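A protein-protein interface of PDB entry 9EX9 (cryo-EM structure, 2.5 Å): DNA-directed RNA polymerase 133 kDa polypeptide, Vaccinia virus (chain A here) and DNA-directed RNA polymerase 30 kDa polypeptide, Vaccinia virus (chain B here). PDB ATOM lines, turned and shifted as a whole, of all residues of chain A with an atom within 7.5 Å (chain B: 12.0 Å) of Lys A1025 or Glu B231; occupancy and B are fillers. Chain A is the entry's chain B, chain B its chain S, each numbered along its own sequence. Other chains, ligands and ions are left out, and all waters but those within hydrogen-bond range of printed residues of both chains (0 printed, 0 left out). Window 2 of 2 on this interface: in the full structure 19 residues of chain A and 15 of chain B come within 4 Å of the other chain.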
ATOM      1  N   TYR A 432     -12.074  10.555 -27.190  1.00  0.00           N
ATOM      2  CA  TYR A 432     -12.423  11.957 -27.384  1.00  0.00           C
ATOM      3  C   TYR A 432     -13.840  12.113 -27.916  1.00  0.00           C
ATOM      4  O   TYR A 432     -14.603  12.951 -27.428  1.00  0.00           O
ATOM      5  CB  TYR A 432     -11.442  12.624 -28.346  1.00  0.00           C
ATOM      6  CG  TYR A 432     -10.022  12.740 -27.852  1.00  0.00           C
ATOM      7  CD1 TYR A 432      -9.720  12.696 -26.501  1.00  0.00           C
ATOM      8  CD2 TYR A 432      -8.979  12.905 -28.746  1.00  0.00           C
ATOM      9  CE1 TYR A 432      -8.422  12.804 -26.060  1.00  0.00           C
ATOM     10  CE2 TYR A 432      -7.681  13.016 -28.316  1.00  0.00           C
ATOM     11  CZ  TYR A 432      -7.406  12.965 -26.972  1.00  0.00           C
ATOM     12  OH  TYR A 432      -6.107  13.077 -26.542  1.00  0.00           O
ATOM     13  N   ARG A 478       0.003  18.980 -38.774  1.00  0.00           N
ATOM     14  CA  ARG A 478       1.326  19.186 -38.201  1.00  0.00           C
ATOM     15  C   ARG A 478       1.780  17.887 -37.551  1.00  0.00           C
ATOM     16  O   ARG A 478       0.985  16.974 -37.315  1.00  0.00           O
ATOM     17  CB  ARG A 478       1.327  20.341 -37.193  1.00  0.00           C
ATOM     18  CG  ARG A 478       0.326  20.190 -36.056  1.00  0.00           C
ATOM     19  CD  ARG A 478       0.129  21.507 -35.317  1.00  0.00           C
ATOM     20  NE  ARG A 478      -0.933  21.434 -34.320  1.00  0.00           N
ATOM     21  CZ  ARG A 478      -0.753  21.153 -33.035  1.00  0.00           C
ATOM     22  NH1 ARG A 478       0.450  20.909 -32.539  1.00  0.00           N
ATOM     23  NH2 ARG A 478      -1.807  21.117 -32.226  1.00  0.00           N
ATOM     24  N   GLN A 696     -12.415  16.609 -32.022  1.00  0.00           N
ATOM     25  CA  GLN A 696     -12.191  16.974 -30.632  1.00  0.00           C
ATOM     26  C   GLN A 696     -13.429  17.535 -29.952  1.00  0.00           C
ATOM     27  O   GLN A 696     -13.384  17.810 -28.752  1.00  0.00           O
ATOM     28  CB  GLN A 696     -11.056  17.989 -30.543  1.00  0.00           C
ATOM     29  CG  GLN A 696      -9.736  17.442 -31.023  1.00  0.00           C
ATOM     30  CD  GLN A 696      -8.616  18.452 -30.962  1.00  0.00           C
ATOM     31  OE1 GLN A 696      -7.489  18.117 -30.606  1.00  0.00           O
ATOM     32  NE2 GLN A 696      -8.911  19.693 -31.322  1.00  0.00           N
ATOM     33  N   MET A 849      -5.815  19.938  -9.560  1.00  0.00           N
ATOM     34  CA  MET A 849      -6.120  21.163  -8.834  1.00  0.00           C
ATOM     35  C   MET A 849      -7.608  21.339  -8.572  1.00  0.00           C
ATOM     36  O   MET A 849      -7.979  22.259  -7.837  1.00  0.00           O
ATOM     37  CB  MET A 849      -5.579  22.376  -9.592  1.00  0.00           C
ATOM     38  CG  MET A 849      -6.163  22.574 -10.970  1.00  0.00           C
ATOM     39  SD  MET A 849      -5.391  23.946 -11.849  1.00  0.00           S
ATOM     40  CE  MET A 849      -6.035  25.355 -10.959  1.00  0.00           C
ATOM     41  N   GLY A 880     -11.057  30.924 -20.469  1.00  0.00           N
ATOM     42  CA  GLY A 880     -10.039  30.115 -21.085  1.00  0.00           C
ATOM     43  C   GLY A 880     -10.552  28.885 -21.805  1.00  0.00           C
ATOM     44  O   GLY A 880      -9.814  28.314 -22.611  1.00  0.00           O
ATOM     45  N   LYS A 882     -12.497  26.521 -24.505  1.00  0.00           N
ATOM     46  CA  LYS A 882     -12.350  26.614 -25.951  1.00  0.00           C
ATOM     47  C   LYS A 882     -13.611  26.116 -26.647  1.00  0.00           C
ATOM     48  O   LYS A 882     -14.122  25.043 -26.315  1.00  0.00           O
ATOM     49  CB  LYS A 882     -11.140  25.795 -26.394  1.00  0.00           C
ATOM     50  CG  LYS A 882     -10.447  26.293 -27.631  1.00  0.00           C
ATOM     51  CD  LYS A 882      -9.164  25.519 -27.864  1.00  0.00           C
ATOM     52  CE  LYS A 882      -8.543  25.859 -29.199  1.00  0.00           C
ATOM     53  NZ  LYS A 882      -7.313  25.070 -29.445  1.00  0.00           N
ATOM     54  N   ARG A1019     -12.156  20.080 -26.172  1.00  0.00           N
ATOM     55  CA  ARG A1019     -11.706  19.392 -24.970  1.00  0.00           C
ATOM     56  C   ARG A1019     -10.534  20.073 -24.279  1.00  0.00           C
ATOM     57  O   ARG A1019     -10.013  19.527 -23.305  1.00  0.00           O
ATOM     58  CB  ARG A1019     -11.317  17.953 -25.305  1.00  0.00           C
ATOM     59  CG  ARG A1019     -10.156  17.853 -26.259  1.00  0.00           C
ATOM     60  CD  ARG A1019      -9.624  16.446 -26.356  1.00  0.00           C
ATOM     61  NE  ARG A1019      -8.405  16.409 -27.151  1.00  0.00           N
ATOM     62  CZ  ARG A1019      -7.193  16.668 -26.680  1.00  0.00           C
ATOM     63  NH1 ARG A1019      -6.995  16.968 -25.408  1.00  0.00           N
ATOM     64  NH2 ARG A1019      -6.153  16.625 -27.507  1.00  0.00           N
ATOM     65  N   HIS A1020     -10.097  21.239 -24.745  1.00  0.00           N
ATOM     66  CA  HIS A1020      -8.974  21.937 -24.133  1.00  0.00           C
ATOM     67  C   HIS A1020      -9.501  22.847 -23.031  1.00  0.00           C
ATOM     68  O   HIS A1020     -10.132  23.869 -23.309  1.00  0.00           O
ATOM     69  CB  HIS A1020      -8.202  22.727 -25.183  1.00  0.00           C
ATOM     70  CG  HIS A1020      -7.582  21.869 -26.241  1.00  0.00           C
ATOM     71  ND1 HIS A1020      -6.381  21.219 -26.062  1.00  0.00           N
ATOM     72  CD2 HIS A1020      -7.999  21.549 -27.488  1.00  0.00           C
ATOM     73  CE1 HIS A1020      -6.083  20.539 -27.153  1.00  0.00           C
ATOM     74  NE2 HIS A1020      -7.049  20.723 -28.034  1.00  0.00           N
ATOM     75  N   LEU A1021      -9.236  22.476 -21.781  1.00  0.00           N
ATOM     76  CA  LEU A1021      -9.733  23.189 -20.614  1.00  0.00           C
ATOM     77  C   LEU A1021      -8.579  23.840 -19.863  1.00  0.00           C
ATOM     78  O   LEU A1021      -7.467  23.310 -19.819  1.00  0.00           O
ATOM     79  CB  LEU A1021     -10.490  22.243 -19.679  1.00  0.00           C
ATOM     80  CG  LEU A1021     -11.544  21.362 -20.342  1.00  0.00           C
ATOM     81  CD1 LEU A1021     -12.208  20.472 -19.320  1.00  0.00           C
ATOM     82  CD2 LEU A1021     -12.570  22.208 -21.046  1.00  0.00           C
ATOM     83  N   THR A1022      -8.861  24.999 -19.267  1.00  0.00           N
ATOM     84  CA  THR A1022      -7.814  25.781 -18.619  1.00  0.00           C
ATOM     85  C   THR A1022      -7.169  25.008 -17.477  1.00  0.00           C
ATOM     86  O   THR A1022      -5.943  24.873 -17.419  1.00  0.00           O
ATOM     87  CB  THR A1022      -8.393  27.097 -18.102  1.00  0.00           C
ATOM     88  OG1 THR A1022      -9.150  27.727 -19.137  1.00  0.00           O
ATOM     89  CG2 THR A1022      -7.287  28.031 -17.656  1.00  0.00           C
ATOM     90  N   GLN A1023      -7.981  24.490 -16.559  1.00  0.00           N
ATOM     91  CA  GLN A1023      -7.445  23.851 -15.367  1.00  0.00           C
ATOM     92  C   GLN A1023      -6.653  22.592 -15.676  1.00  0.00           C
ATOM     93  O   GLN A1023      -5.920  22.117 -14.806  1.00  0.00           O
ATOM     94  CB  GLN A1023      -8.577  23.527 -14.398  1.00  0.00           C
ATOM     95  CG  GLN A1023      -9.187  24.751 -13.766  1.00  0.00           C
ATOM     96  CD  GLN A1023     -10.221  24.413 -12.727  1.00  0.00           C
ATOM     97  OE1 GLN A1023     -10.621  23.264 -12.588  1.00  0.00           O
ATOM     98  NE2 GLN A1023     -10.660  25.416 -11.984  1.00  0.00           N
ATOM     99  N   ASP A1024      -6.779  22.042 -16.878  1.00  0.00           N
ATOM    100  CA  ASP A1024      -5.935  20.931 -17.284  1.00  0.00           C
ATOM    101  C   ASP A1024      -4.560  21.384 -17.749  1.00  0.00           C
ATOM    102  O   ASP A1024      -3.688  20.536 -17.960  1.00  0.00           O
ATOM    103  CB  ASP A1024      -6.611  20.137 -18.402  1.00  0.00           C
ATOM    104  CG  ASP A1024      -7.914  19.510 -17.964  1.00  0.00           C
ATOM    105  OD1 ASP A1024      -8.345  19.765 -16.824  1.00  0.00           O
ATOM    106  OD2 ASP A1024      -8.509  18.757 -18.759  1.00  0.00           O
ATOM    107  N   LYS A1025      -4.345  22.688 -17.912  1.00  0.00           N
ATOM    108  CA  LYS A1025      -3.080  23.215 -18.393  1.00  0.00           C
ATOM    109  C   LYS A1025      -2.375  24.110 -17.387  1.00  0.00           C
ATOM    110  O   LYS A1025      -1.220  24.482 -17.622  1.00  0.00           O
ATOM    111  CB  LYS A1025      -3.294  24.004 -19.692  1.00  0.00           C
ATOM    112  CG  LYS A1025      -4.009  23.219 -20.776  1.00  0.00           C
ATOM    113  CD  LYS A1025      -4.439  24.118 -21.913  1.00  0.00           C
ATOM    114  CE  LYS A1025      -5.217  23.354 -22.961  1.00  0.00           C
ATOM    115  NZ  LYS A1025      -4.385  22.319 -23.622  1.00  0.00           N
ATOM    116  N   ALA A1026      -3.025  24.464 -16.284  1.00  0.00           N
ATOM    117  CA  ALA A1026      -2.413  25.331 -15.291  1.00  0.00           C
ATOM    118  C   ALA A1026      -1.258  24.628 -14.593  1.00  0.00           C
ATOM    119  O   ALA A1026      -1.294  23.416 -14.364  1.00  0.00           O
ATOM    120  CB  ALA A1026      -3.457  25.762 -14.268  1.00  0.00           C
ATOM    121  N   THR A1027      -0.228  25.396 -14.248  1.00  0.00           N
ATOM    122  CA  THR A1027       0.940  24.858 -13.569  1.00  0.00           C
ATOM    123  C   THR A1027       1.607  25.968 -12.772  1.00  0.00           C
ATOM    124  O   THR A1027       1.655  27.119 -13.208  1.00  0.00           O
ATOM    125  CB  THR A1027       1.935  24.259 -14.565  1.00  0.00           C
ATOM    126  OG1 THR A1027       1.240  23.404 -15.479  1.00  0.00           O
ATOM    127  CG2 THR A1027       2.998  23.457 -13.844  1.00  0.00           C
ATOM    128  N   VAL A1028       2.127  25.610 -11.600  1.00  0.00           N
ATOM    129  CA  VAL A1028       2.840  26.555 -10.746  1.00  0.00           C
ATOM    130  C   VAL A1028       3.771  25.763  -9.843  1.00  0.00           C
ATOM    131  O   VAL A1028       3.443  24.657  -9.408  1.00  0.00           O
ATOM    132  CB  VAL A1028       1.860  27.429  -9.927  1.00  0.00           C
ATOM    133  CG1 VAL A1028       0.985  26.567  -9.039  1.00  0.00           C
ATOM    134  CG2 VAL A1028       2.617  28.447  -9.096  1.00  0.00           C
ATOM    135  N   ARG A1045       4.359  17.782 -15.008  1.00  0.00           N
ATOM    136  CA  ARG A1045       3.288  18.555 -14.390  1.00  0.00           C
ATOM    137  C   ARG A1045       2.630  17.770 -13.264  1.00  0.00           C
ATOM    138  O   ARG A1045       2.317  18.328 -12.207  1.00  0.00           O
ATOM    139  CB  ARG A1045       2.258  18.953 -15.443  1.00  0.00           C
ATOM    140  CG  ARG A1045       1.093  19.740 -14.887  1.00  0.00           C
ATOM    141  CD  ARG A1045       0.119  20.153 -15.968  1.00  0.00           C
ATOM    142  NE  ARG A1045      -1.032  20.832 -15.389  1.00  0.00           N
ATOM    143  CZ  ARG A1045      -2.105  20.217 -14.913  1.00  0.00           C
ATOM    144  NH1 ARG A1045      -2.233  18.901 -14.973  1.00  0.00           N
ATOM    145  NH2 ARG A1045      -3.074  20.939 -14.359  1.00  0.00           N
ATOM    146  N   PRO B 227       0.647  26.948 -34.388  1.00  0.00           N
ATOM    147  CA  PRO B 227       0.309  25.651 -33.796  1.00  0.00           C
ATOM    148  C   PRO B 227       0.043  25.729 -32.299  1.00  0.00           C
ATOM    149  O   PRO B 227       0.825  26.326 -31.564  1.00  0.00           O
ATOM    150  CB  PRO B 227       1.549  24.803 -34.082  1.00  0.00           C
ATOM    151  CG  PRO B 227       2.651  25.778 -34.212  1.00  0.00           C
ATOM    152  CD  PRO B 227       2.048  26.995 -34.838  1.00  0.00           C
ATOM    153  N   SEP B 228      -1.057  25.127 -31.861  1.00  0.00           N
ATOM    154  CA  SEP B 228      -1.405  25.100 -30.449  1.00  0.00           C
ATOM    155  CB  SEP B 228      -2.651  24.248 -30.231  1.00  0.00           C
ATOM    156  OG  SEP B 228      -3.753  24.782 -30.940  1.00  0.00           O
ATOM    157  C   SEP B 228      -0.248  24.555 -29.619  1.00  0.00           C
ATOM    158  O   SEP B 228       0.569  23.790 -30.127  1.00  0.00           O
ATOM    159  P   SEP B 228      -4.517  23.653 -31.797  1.00  0.00           P
ATOM    160  O1P SEP B 228      -3.806  23.504 -33.232  1.00  0.00           O
ATOM    161  O2P SEP B 228      -4.490  22.242 -31.025  1.00  0.00           O
ATOM    162  O3P SEP B 228      -6.044  24.105 -32.015  1.00  0.00           O
ATOM    163  N   PRO B 229      -0.169  24.944 -28.336  1.00  0.00           N
ATOM    164  CA  PRO B 229       0.931  24.453 -27.501  1.00  0.00           C
ATOM    165  C   PRO B 229       0.920  22.930 -27.340  1.00  0.00           C
ATOM    166  O   PRO B 229      -0.162  22.347 -27.275  1.00  0.00           O
ATOM    167  CB  PRO B 229       0.684  25.139 -26.154  1.00  0.00           C
ATOM    168  CG  PRO B 229      -0.190  26.295 -26.457  1.00  0.00           C
ATOM    169  CD  PRO B 229      -1.045  25.868 -27.598  1.00  0.00           C
ATOM    170  N   PRO B 230       2.092  22.296 -27.271  1.00  0.00           N
ATOM    171  CA  PRO B 230       2.127  20.835 -27.120  1.00  0.00           C
ATOM    172  C   PRO B 230       1.602  20.412 -25.756  1.00  0.00           C
ATOM    173  O   PRO B 230       1.855  21.075 -24.748  1.00  0.00           O
ATOM    174  CB  PRO B 230       3.614  20.489 -27.281  1.00  0.00           C
ATOM    175  CG  PRO B 230       4.282  21.746 -27.755  1.00  0.00           C
ATOM    176  CD  PRO B 230       3.447  22.869 -27.261  1.00  0.00           C
ATOM    177  N   GLU B 231       0.875  19.301 -25.730  1.00  0.00           N
ATOM    178  CA  GLU B 231       0.409  18.721 -24.476  1.00  0.00           C
ATOM    179  C   GLU B 231       1.450  17.753 -23.933  1.00  0.00           C
ATOM    180  O   GLU B 231       2.416  17.422 -24.621  1.00  0.00           O
ATOM    181  CB  GLU B 231      -0.922  17.998 -24.670  1.00  0.00           C
ATOM    182  CG  GLU B 231      -2.086  18.907 -25.005  1.00  0.00           C
ATOM    183  CD  GLU B 231      -3.388  18.145 -25.158  1.00  0.00           C
ATOM    184  OE1 GLU B 231      -3.335  16.909 -25.327  1.00  0.00           O
ATOM    185  OE2 GLU B 231      -4.461  18.779 -25.106  1.00  0.00           O
ATOM    186  N   SEP B 232       1.257  17.301 -22.701  1.00  0.00           N
ATOM    187  CA  SEP B 232       2.177  16.348 -22.097  1.00  0.00           C
ATOM    188  CB  SEP B 232       1.774  16.053 -20.652  1.00  0.00           C
ATOM    189  OG  SEP B 232       1.831  17.235 -19.874  1.00  0.00           O
ATOM    190  C   SEP B 232       2.206  15.063 -22.925  1.00  0.00           C
ATOM    191  O   SEP B 232       1.156  14.584 -23.356  1.00  0.00           O
ATOM    192  P   SEP B 232       3.101  17.199 -18.889  1.00  0.00           P
ATOM    193  O1P SEP B 232       3.394  18.685 -18.341  1.00  0.00           O
ATOM    194  O2P SEP B 232       4.397  16.662 -19.678  1.00  0.00           O
ATOM    195  O3P SEP B 232       2.773  16.215 -17.659  1.00  0.00           O
ATOM    196  N   PRO B 233       3.407  14.506 -23.165  1.00  0.00           N
ATOM    197  CA  PRO B 233       3.515  13.293 -23.986  1.00  0.00           C
ATOM    198  C   PRO B 233       2.553  12.198 -23.541  1.00  0.00           C
ATOM    199  O   PRO B 233       1.706  11.771 -24.324  1.00  0.00           O
ATOM    200  CB  PRO B 233       4.971  12.863 -23.785  1.00  0.00           C
ATOM    201  CG  PRO B 233       5.688  14.113 -23.451  1.00  0.00           C
ATOM    202  CD  PRO B 233       4.722  14.953 -22.675  1.00  0.00           C
ATOM    203  N   GLU B 234       2.686  11.762 -22.293  1.00  0.00           N
ATOM    204  CA  GLU B 234       1.781  10.776 -21.712  1.00  0.00           C
ATOM    205  C   GLU B 234       1.574   9.585 -22.642  1.00  0.00           C
ATOM    206  O   GLU B 234       2.146   8.516 -22.430  1.00  0.00           O
ATOM    207  CB  GLU B 234       0.435  11.428 -21.385  1.00  0.00           C
ATOM    208  CG  GLU B 234       0.559  12.706 -20.567  1.00  0.00           C
ATOM    209  CD  GLU B 234      -0.545  12.860 -19.538  1.00  0.00           C
ATOM    210  OE1 GLU B 234      -1.637  12.286 -19.738  1.00  0.00           O
ATOM    211  OE2 GLU B 234      -0.317  13.553 -18.523  1.00  0.00           O
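Of the 17 printed residues of chain A, 6 touch a printed residue of chain B.
Hydrophobic or aromatic side chains of chain B that line the printed part of chain A: Pro B227.
Among the printed residues, Asp or Glu carboxylates within 4 Å of a Lys or Arg side-chain nitrogen of the other chain: Arg A1019 with Glu B231 (3.1 Å) and Lys A1025 with Glu B231 (3.8 Å).
The guanidinium group (NH1) of Arg A1019 lies within salt-bridge range of the side-chain carboxylate (OE2) of Glu B231, at 3.1 Å.
The side-chain carboxylate (OE2) of Glu B231 lies within salt-bridge range of the side-chain amino group (NZ) of Lys A1025 (3.8 Å).
O3P of SEP B232 is in hydrogen-bond range of the backbone NH of Arg A1045, 3.5 Å away.
O2P of SEP B228 lies close to NH2 of Arg A478 (3.1 Å).
OE2 of Glu B231 sits close to ND1 of His A1020 (3.2 Å).
O3P of SEP B228 lies close to the side-chain amino group of Lys A882, at 3.0 Å.
CD of Arg A478 touches CB of Pro B227 (3.8 Å).
OG1 of Thr A1027 sits at hydrogen-bond distance from NE of Arg A1045 (3.4 Å).
O of Lys A1025 sits at hydrogen-bond distance from OG1 of Thr A1027, at 3.4 Å.
O of Gln A1023 lies within hydrogen-bond range of NH2 of Arg A1045.
ND1 of His A1020 is in hydrogen-bond range of NZ of Lys A1025 (3.3 Å).
The backbone carbonyl oxygen of Ala A1026 sits at hydrogen-bond distance from the guanidinium group of Arg A1045, at 2.8 Å.
Tyr A432 touches none of the printed residues of chain B.
No residue of chain B comes within 4 Å of Thr A1022.
No residue of chain B comes within 4 Å of Thr A1027.
Of the printed residues of chain B, Arg A1045 touches SEP B232 (3.1 Å).
Glu B231 touches three residues of chain A.
Of the printed residues of chain A, SEP B232 touches Arg A1045 (3.1 Å).
Pro B233 touches none of the printed residues of chain A.
The nearest residue of chain B that does not touch Lys A1025 is Pro B229 (5.6 Å).
The nearest residue of chain A that does not touch Glu B231 is Tyr A432 (4.9 Å).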
